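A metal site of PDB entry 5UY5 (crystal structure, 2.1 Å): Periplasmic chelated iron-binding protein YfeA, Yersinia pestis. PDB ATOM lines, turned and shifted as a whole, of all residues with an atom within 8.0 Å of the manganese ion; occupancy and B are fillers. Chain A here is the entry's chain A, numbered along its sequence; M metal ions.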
ATOM      1  N   GLU A  74      19.233  20.632  -2.461  1.00  0.00           N
ATOM      2  CA  GLU A  74      19.751  19.275  -2.598  1.00  0.00           C
ATOM      3  C   GLU A  74      18.918  18.306  -1.763  1.00  0.00           C
ATOM      4  O   GLU A  74      18.770  18.484  -0.546  1.00  0.00           O
ATOM      5  CB  GLU A  74      21.217  19.256  -2.165  1.00  0.00           C
ATOM      6  CG  GLU A  74      22.088  18.165  -2.753  1.00  0.00           C
ATOM      7  CD  GLU A  74      21.695  16.783  -2.237  1.00  0.00           C
ATOM      8  OE1 GLU A  74      21.694  16.569  -1.007  1.00  0.00           O
ATOM      9  OE2 GLU A  74      21.342  15.922  -3.083  1.00  0.00           O
ATOM     10  N   ILE A  75      18.390  17.262  -2.388  1.00  0.00           N
ATOM     11  CA  ILE A  75      17.344  16.437  -1.778  1.00  0.00           C
ATOM     12  C   ILE A  75      17.873  15.169  -1.123  1.00  0.00           C
ATOM     13  O   ILE A  75      17.220  14.603  -0.245  1.00  0.00           O
ATOM     14  CB  ILE A  75      16.282  16.067  -2.826  1.00  0.00           C
ATOM     15  CG1 ILE A  75      16.944  15.304  -3.981  1.00  0.00           C
ATOM     16  CG2 ILE A  75      15.582  17.299  -3.351  1.00  0.00           C
ATOM     17  CD1 ILE A  75      15.891  14.760  -4.999  1.00  0.00           C
ATOM     18  N   HIS A  76      19.029  14.677  -1.568  1.00  0.00           N
ATOM     19  CA  HIS A  76      19.530  13.396  -1.071  1.00  0.00           C
ATOM     20  C   HIS A  76      19.856  13.484   0.418  1.00  0.00           C
ATOM     21  O   HIS A  76      19.476  12.610   1.201  1.00  0.00           O
ATOM     22  CB  HIS A  76      20.757  12.958  -1.856  1.00  0.00           C
ATOM     23  CG  HIS A  76      20.488  12.635  -3.300  1.00  0.00           C
ATOM     24  ND1 HIS A  76      20.365  11.333  -3.757  1.00  0.00           N
ATOM     25  CD2 HIS A  76      20.377  13.435  -4.382  1.00  0.00           C
ATOM     26  CE1 HIS A  76      20.171  11.354  -5.064  1.00  0.00           C
ATOM     27  NE2 HIS A  76      20.160  12.618  -5.466  1.00  0.00           N
ATOM     28  N   LEU A 101      16.091   7.421  -1.949  1.00  0.00           N
ATOM     29  CA  LEU A 101      16.455   8.747  -2.449  1.00  0.00           C
ATOM     30  C   LEU A 101      16.691   9.702  -1.287  1.00  0.00           C
ATOM     31  O   LEU A 101      17.774  10.311  -1.167  1.00  0.00           O
ATOM     32  CB  LEU A 101      15.357   9.291  -3.376  1.00  0.00           C
ATOM     33  CG  LEU A 101      15.552  10.776  -3.742  1.00  0.00           C
ATOM     34  CD1 LEU A 101      16.810  10.933  -4.615  1.00  0.00           C
ATOM     35  CD2 LEU A 101      14.350  11.333  -4.463  1.00  0.00           C
ATOM     36  N   ASN A 139      19.657   3.000  -7.968  1.00  0.00           N
ATOM     37  CA  ASN A 139      19.727   4.382  -8.443  1.00  0.00           C
ATOM     38  C   ASN A 139      18.334   4.964  -8.277  1.00  0.00           C
ATOM     39  O   ASN A 139      17.385   4.433  -8.870  1.00  0.00           O
ATOM     40  CB  ASN A 139      20.166   4.424  -9.904  1.00  0.00           C
ATOM     41  CG  ASN A 139      20.403   5.830 -10.415  1.00  0.00           C
ATOM     42  OD1 ASN A 139      19.673   6.779 -10.079  1.00  0.00           O
ATOM     43  ND2 ASN A 139      21.436   5.971 -11.257  1.00  0.00           N
ATOM     44  N   PRO A 140      18.151   6.017  -7.464  1.00  0.00           N
ATOM     45  CA  PRO A 140      16.795   6.459  -7.101  1.00  0.00           C
ATOM     46  C   PRO A 140      16.107   7.317  -8.154  1.00  0.00           C
ATOM     47  O   PRO A 140      14.893   7.560  -8.032  1.00  0.00           O
ATOM     48  CB  PRO A 140      17.029   7.263  -5.817  1.00  0.00           C
ATOM     49  CG  PRO A 140      18.437   7.830  -5.989  1.00  0.00           C
ATOM     50  CD  PRO A 140      19.199   6.798  -6.766  1.00  0.00           C
ATOM     51  N   HIS A 141      16.822   7.738  -9.206  1.00  0.00           N
ATOM     52  CA  HIS A 141      16.335   8.748 -10.133  1.00  0.00           C
ATOM     53  C   HIS A 141      15.420   8.162 -11.203  1.00  0.00           C
ATOM     54  O   HIS A 141      15.587   8.456 -12.396  1.00  0.00           O
ATOM     55  CB  HIS A 141      17.526   9.455 -10.811  1.00  0.00           C
ATOM     56  CG  HIS A 141      18.500  10.062  -9.856  1.00  0.00           C
ATOM     57  ND1 HIS A 141      19.683   9.438  -9.507  1.00  0.00           N
ATOM     58  CD2 HIS A 141      18.467  11.226  -9.167  1.00  0.00           C
ATOM     59  CE1 HIS A 141      20.343  10.204  -8.641  1.00  0.00           C
ATOM     60  NE2 HIS A 141      19.622  11.290  -8.415  1.00  0.00           N
ATOM     61  N   TRP A 143      12.385   8.732 -12.052  1.00  0.00           N
ATOM     62  CA  TRP A 143      11.490   9.654 -12.754  1.00  0.00           C
ATOM     63  C   TRP A 143      12.088  10.197 -14.048  1.00  0.00           C
ATOM     64  O   TRP A 143      11.333  10.759 -14.848  1.00  0.00           O
ATOM     65  CB  TRP A 143      11.085  10.820 -11.848  1.00  0.00           C
ATOM     66  CG  TRP A 143      12.232  11.682 -11.439  1.00  0.00           C
ATOM     67  CD1 TRP A 143      12.691  12.787 -12.093  1.00  0.00           C
ATOM     68  CD2 TRP A 143      13.068  11.518 -10.278  1.00  0.00           C
ATOM     69  NE1 TRP A 143      13.773  13.331 -11.410  1.00  0.00           N
ATOM     70  CE2 TRP A 143      14.013  12.563 -10.295  1.00  0.00           C
ATOM     71  CE3 TRP A 143      13.085  10.603  -9.234  1.00  0.00           C
ATOM     72  CZ2 TRP A 143      14.980  12.693  -9.307  1.00  0.00           C
ATOM     73  CZ3 TRP A 143      14.033  10.743  -8.238  1.00  0.00           C
ATOM     74  CH2 TRP A 143      14.976  11.792  -8.284  1.00  0.00           C
ATOM     75  N   GLU A 207      26.535  14.283 -11.228  1.00  0.00           N
ATOM     76  CA  GLU A 207      25.922  13.107 -10.607  1.00  0.00           C
ATOM     77  C   GLU A 207      25.501  12.116 -11.702  1.00  0.00           C
ATOM     78  O   GLU A 207      25.066  12.511 -12.776  1.00  0.00           O
ATOM     79  CB  GLU A 207      24.706  13.509  -9.752  1.00  0.00           C
ATOM     80  CG  GLU A 207      24.113  12.355  -8.938  1.00  0.00           C
ATOM     81  CD  GLU A 207      22.840  12.689  -8.172  1.00  0.00           C
ATOM     82  OE1 GLU A 207      22.096  13.620  -8.552  1.00  0.00           O
ATOM     83  OE2 GLU A 207      22.559  11.996  -7.180  1.00  0.00           O
ATOM     84  N   GLY A 208      25.656  10.818 -11.416  1.00  0.00           N
ATOM     85  CA  GLY A 208      25.137   9.775 -12.290  1.00  0.00           C
ATOM     86  C   GLY A 208      23.624   9.637 -12.146  1.00  0.00           C
ATOM     87  O   GLY A 208      23.089   8.544 -11.919  1.00  0.00           O
ATOM     88  N   ALA A 209      22.925  10.756 -12.310  1.00  0.00           N
ATOM     89  CA  ALA A 209      21.496  10.851 -12.055  1.00  0.00           C
ATOM     90  C   ALA A 209      20.647  10.541 -13.280  1.00  0.00           C
ATOM     91  O   ALA A 209      19.413  10.578 -13.186  1.00  0.00           O
ATOM     92  CB  ALA A 209      21.163  12.248 -11.524  1.00  0.00           C
ATOM     93  N   PHE A 210      21.268  10.222 -14.411  1.00  0.00           N
ATOM     94  CA  PHE A 210      20.514  10.141 -15.660  1.00  0.00           C
ATOM     95  C   PHE A 210      20.439   8.727 -16.207  1.00  0.00           C
ATOM     96  O   PHE A 210      20.043   8.549 -17.366  1.00  0.00           O
ATOM     97  CB  PHE A 210      21.103  11.102 -16.670  1.00  0.00           C
ATOM     98  CG  PHE A 210      21.029  12.518 -16.222  1.00  0.00           C
ATOM     99  CD1 PHE A 210      19.908  13.294 -16.518  1.00  0.00           C
ATOM    100  CD2 PHE A 210      22.037  13.061 -15.424  1.00  0.00           C
ATOM    101  CE1 PHE A 210      19.813  14.615 -16.076  1.00  0.00           C
ATOM    102  CE2 PHE A 210      21.950  14.367 -14.971  1.00  0.00           C
ATOM    103  CZ  PHE A 210      20.824  15.154 -15.302  1.00  0.00           C
ATOM    104  N   TRP A 225      30.424  11.640 -10.113  1.00  0.00           N
ATOM    105  CA  TRP A 225      30.197  10.824  -8.930  1.00  0.00           C
ATOM    106  C   TRP A 225      28.894  10.065  -9.091  1.00  0.00           C
ATOM    107  O   TRP A 225      27.955  10.578  -9.718  1.00  0.00           O
ATOM    108  CB  TRP A 225      30.185  11.677  -7.641  1.00  0.00           C
ATOM    109  CG  TRP A 225      29.229  12.840  -7.642  1.00  0.00           C
ATOM    110  CD1 TRP A 225      27.916  12.825  -7.250  1.00  0.00           C
ATOM    111  CD2 TRP A 225      29.514  14.187  -8.031  1.00  0.00           C
ATOM    112  NE1 TRP A 225      27.373  14.087  -7.378  1.00  0.00           N
ATOM    113  CE2 TRP A 225      28.333  14.938  -7.866  1.00  0.00           C
ATOM    114  CE3 TRP A 225      30.658  14.839  -8.525  1.00  0.00           C
ATOM    115  CZ2 TRP A 225      28.262  16.297  -8.160  1.00  0.00           C
ATOM    116  CZ3 TRP A 225      30.580  16.182  -8.817  1.00  0.00           C
ATOM    117  CH2 TRP A 225      29.398  16.903  -8.638  1.00  0.00           C
ATOM    118  N   PRO A 226      28.796   8.846  -8.564  1.00  0.00           N
ATOM    119  CA  PRO A 226      27.647   8.008  -8.940  1.00  0.00           C
ATOM    120  C   PRO A 226      26.328   8.437  -8.301  1.00  0.00           C
ATOM    121  O   PRO A 226      25.281   8.302  -8.949  1.00  0.00           O
ATOM    122  CB  PRO A 226      28.080   6.596  -8.500  1.00  0.00           C
ATOM    123  CG  PRO A 226      29.264   6.790  -7.599  1.00  0.00           C
ATOM    124  CD  PRO A 226      29.907   8.083  -7.964  1.00  0.00           C
ATOM    125  N   ILE A 227      26.346   8.987  -7.090  1.00  0.00           N
ATOM    126  CA  ILE A 227      25.141   9.499  -6.433  1.00  0.00           C
ATOM    127  C   ILE A 227      25.570  10.599  -5.464  1.00  0.00           C
ATOM    128  O   ILE A 227      26.638  10.512  -4.855  1.00  0.00           O
ATOM    129  CB  ILE A 227      24.353   8.369  -5.712  1.00  0.00           C
ATOM    130  CG1 ILE A 227      23.094   8.923  -5.037  1.00  0.00           C
ATOM    131  CG2 ILE A 227      25.239   7.639  -4.687  1.00  0.00           C
ATOM    132  CD1 ILE A 227      22.097   7.847  -4.625  1.00  0.00           C
ATOM    133  N   ASN A 228      24.747  11.649  -5.343  1.00  0.00           N
ATOM    134  CA  ASN A 228      25.044  12.723  -4.413  1.00  0.00           C
ATOM    135  C   ASN A 228      25.203  12.150  -3.014  1.00  0.00           C
ATOM    136  O   ASN A 228      24.378  11.335  -2.579  1.00  0.00           O
ATOM    137  CB  ASN A 228      23.934  13.770  -4.381  1.00  0.00           C
ATOM    138  CG  ASN A 228      23.873  14.609  -5.619  1.00  0.00           C
ATOM    139  OD1 ASN A 228      24.742  14.540  -6.492  1.00  0.00           O
ATOM    140  ND2 ASN A 228      22.804  15.411  -5.720  1.00  0.00           N
ATOM    141  N   ALA A 229      26.252  12.574  -2.324  1.00  0.00           N
ATOM    142  CA  ALA A 229      26.547  12.184  -0.946  1.00  0.00           C
ATOM    143  C   ALA A 229      27.826  12.905  -0.540  1.00  0.00           C
ATOM    144  O   ALA A 229      28.528  13.472  -1.377  1.00  0.00           O
ATOM    145  CB  ALA A 229      26.722  10.666  -0.783  1.00  0.00           C
ATOM    146  N   GLU A 256      24.424  19.819 -12.913  1.00  0.00           N
ATOM    147  CA  GLU A 256      23.018  19.762 -12.555  1.00  0.00           C
ATOM    148  C   GLU A 256      22.658  20.876 -11.587  1.00  0.00           C
ATOM    149  O   GLU A 256      23.512  21.411 -10.878  1.00  0.00           O
ATOM    150  CB  GLU A 256      22.655  18.413 -11.926  1.00  0.00           C
ATOM    151  CG  GLU A 256      22.877  17.235 -12.856  1.00  0.00           C
ATOM    152  CD  GLU A 256      24.255  16.617 -12.672  1.00  0.00           C
ATOM    153  OE1 GLU A 256      24.638  16.342 -11.515  1.00  0.00           O
ATOM    154  OE2 GLU A 256      24.968  16.418 -13.688  1.00  0.00           O
ATOM    155  N   THR A 258      21.152  21.273  -8.702  1.00  0.00           N
ATOM    156  CA  THR A 258      21.243  21.337  -7.239  1.00  0.00           C
ATOM    157  C   THR A 258      22.658  21.121  -6.714  1.00  0.00           C
ATOM    158  O   THR A 258      22.845  21.053  -5.500  1.00  0.00           O
ATOM    159  CB  THR A 258      20.305  20.324  -6.571  1.00  0.00           C
ATOM    160  OG1 THR A 258      20.765  18.985  -6.790  1.00  0.00           O
ATOM    161  CG2 THR A 258      18.883  20.460  -7.091  1.00  0.00           C
ATOM    162  N   ILE A 259      23.659  21.027  -7.597  1.00  0.00           N
ATOM    163  CA  ILE A 259      25.026  20.768  -7.185  1.00  0.00           C
ATOM    164  C   ILE A 259      25.968  21.738  -7.911  1.00  0.00           C
ATOM    165  O   ILE A 259      25.577  22.450  -8.829  1.00  0.00           O
ATOM    166  CB  ILE A 259      25.429  19.297  -7.435  1.00  0.00           C
ATOM    167  CG1 ILE A 259      25.012  18.837  -8.842  1.00  0.00           C
ATOM    168  CG2 ILE A 259      24.780  18.369  -6.398  1.00  0.00           C
ATOM    169  CD1 ILE A 259      26.025  19.185  -9.946  1.00  0.00           C
ATOM    170  N   VAL A 281      17.379  17.529 -12.783  1.00  0.00           N
ATOM    171  CA  VAL A 281      16.970  16.172 -12.435  1.00  0.00           C
ATOM    172  C   VAL A 281      16.354  16.116 -11.040  1.00  0.00           C
ATOM    173  O   VAL A 281      15.246  15.606 -10.858  1.00  0.00           O
ATOM    174  CB  VAL A 281      18.143  15.178 -12.559  1.00  0.00           C
ATOM    175  CG1 VAL A 281      19.362  15.672 -11.798  1.00  0.00           C
ATOM    176  CG2 VAL A 281      17.736  13.795 -12.052  1.00  0.00           C
ATOM    177  N   ASP A 282      17.061  16.651 -10.047  1.00  0.00           N
ATOM    178  CA  ASP A 282      16.667  16.514  -8.649  1.00  0.00           C
ATOM    179  C   ASP A 282      15.696  17.585  -8.182  1.00  0.00           C
ATOM    180  O   ASP A 282      15.123  17.449  -7.094  1.00  0.00           O
ATOM    181  CB  ASP A 282      17.898  16.556  -7.747  1.00  0.00           C
ATOM    182  CG  ASP A 282      18.652  15.257  -7.763  1.00  0.00           C
ATOM    183  OD1 ASP A 282      18.099  14.266  -8.320  1.00  0.00           O
ATOM    184  OD2 ASP A 282      19.773  15.226  -7.218  1.00  0.00           O
ATOM    185  N   SER A 283      15.501  18.648  -8.959  1.00  0.00           N
ATOM    186  CA  SER A 283      14.607  19.704  -8.525  1.00  0.00           C
ATOM    187  C   SER A 283      14.053  20.423  -9.735  1.00  0.00           C
ATOM    188  O   SER A 283      14.729  20.564 -10.758  1.00  0.00           O
ATOM    189  CB  SER A 283      15.320  20.705  -7.596  1.00  0.00           C
ATOM    190  OG  SER A 283      14.479  21.815  -7.333  1.00  0.00           O
HETATM  191 MN    MN M   1      20.311  13.127  -7.421  1.00  0.00          MN
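OD2 of Asp 282 sits close to ND2 of Asn 228 (3.4 Å).
OE2 of Glu 207 sits close to N of Asn 228 (2.9 Å).
The backbone NH (N) of His 76 lies close to the side-chain carboxylate (OE2) of Glu 74, 3.0 Å away.
N of Glu 207 sits at hydrogen-bond distance from OE1 of Glu 256 (2.8 Å).
The side-chain amide nitrogen of Asn 228 is in hydrogen-bond range of the side-chain carboxylate of Glu 74, 3.1 Å away.
NE1 of Trp 225 lies within hydrogen-bond range of OD1 of Asn 228, at 2.8 Å.
A ring nitrogen (ND1) of His 141 is in hydrogen-bond range of the side-chain amide oxygen of Asn 139 (2.7 Å).
Asn 228 touches the manganese ion (ND2 to MN, 3.8 Å).
Of the 23 residues printed, 5 come within 4 Å of the manganese ion.
The nearest printed residue that does not touch the manganese ion is Ala 209 (4.3 Å).
The manganese ion is bound by a ring nitrogen (NE2) of His 76, the side-chain carboxylate (OE1) of Glu 207, the side-chain carboxylate (OD2) of Asp 282, a ring nitrogen (NE2) of His 141, the side-chain carboxylate (OE2) of Glu 207 and the side-chain carboxylate (OD1) of Asp 282.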
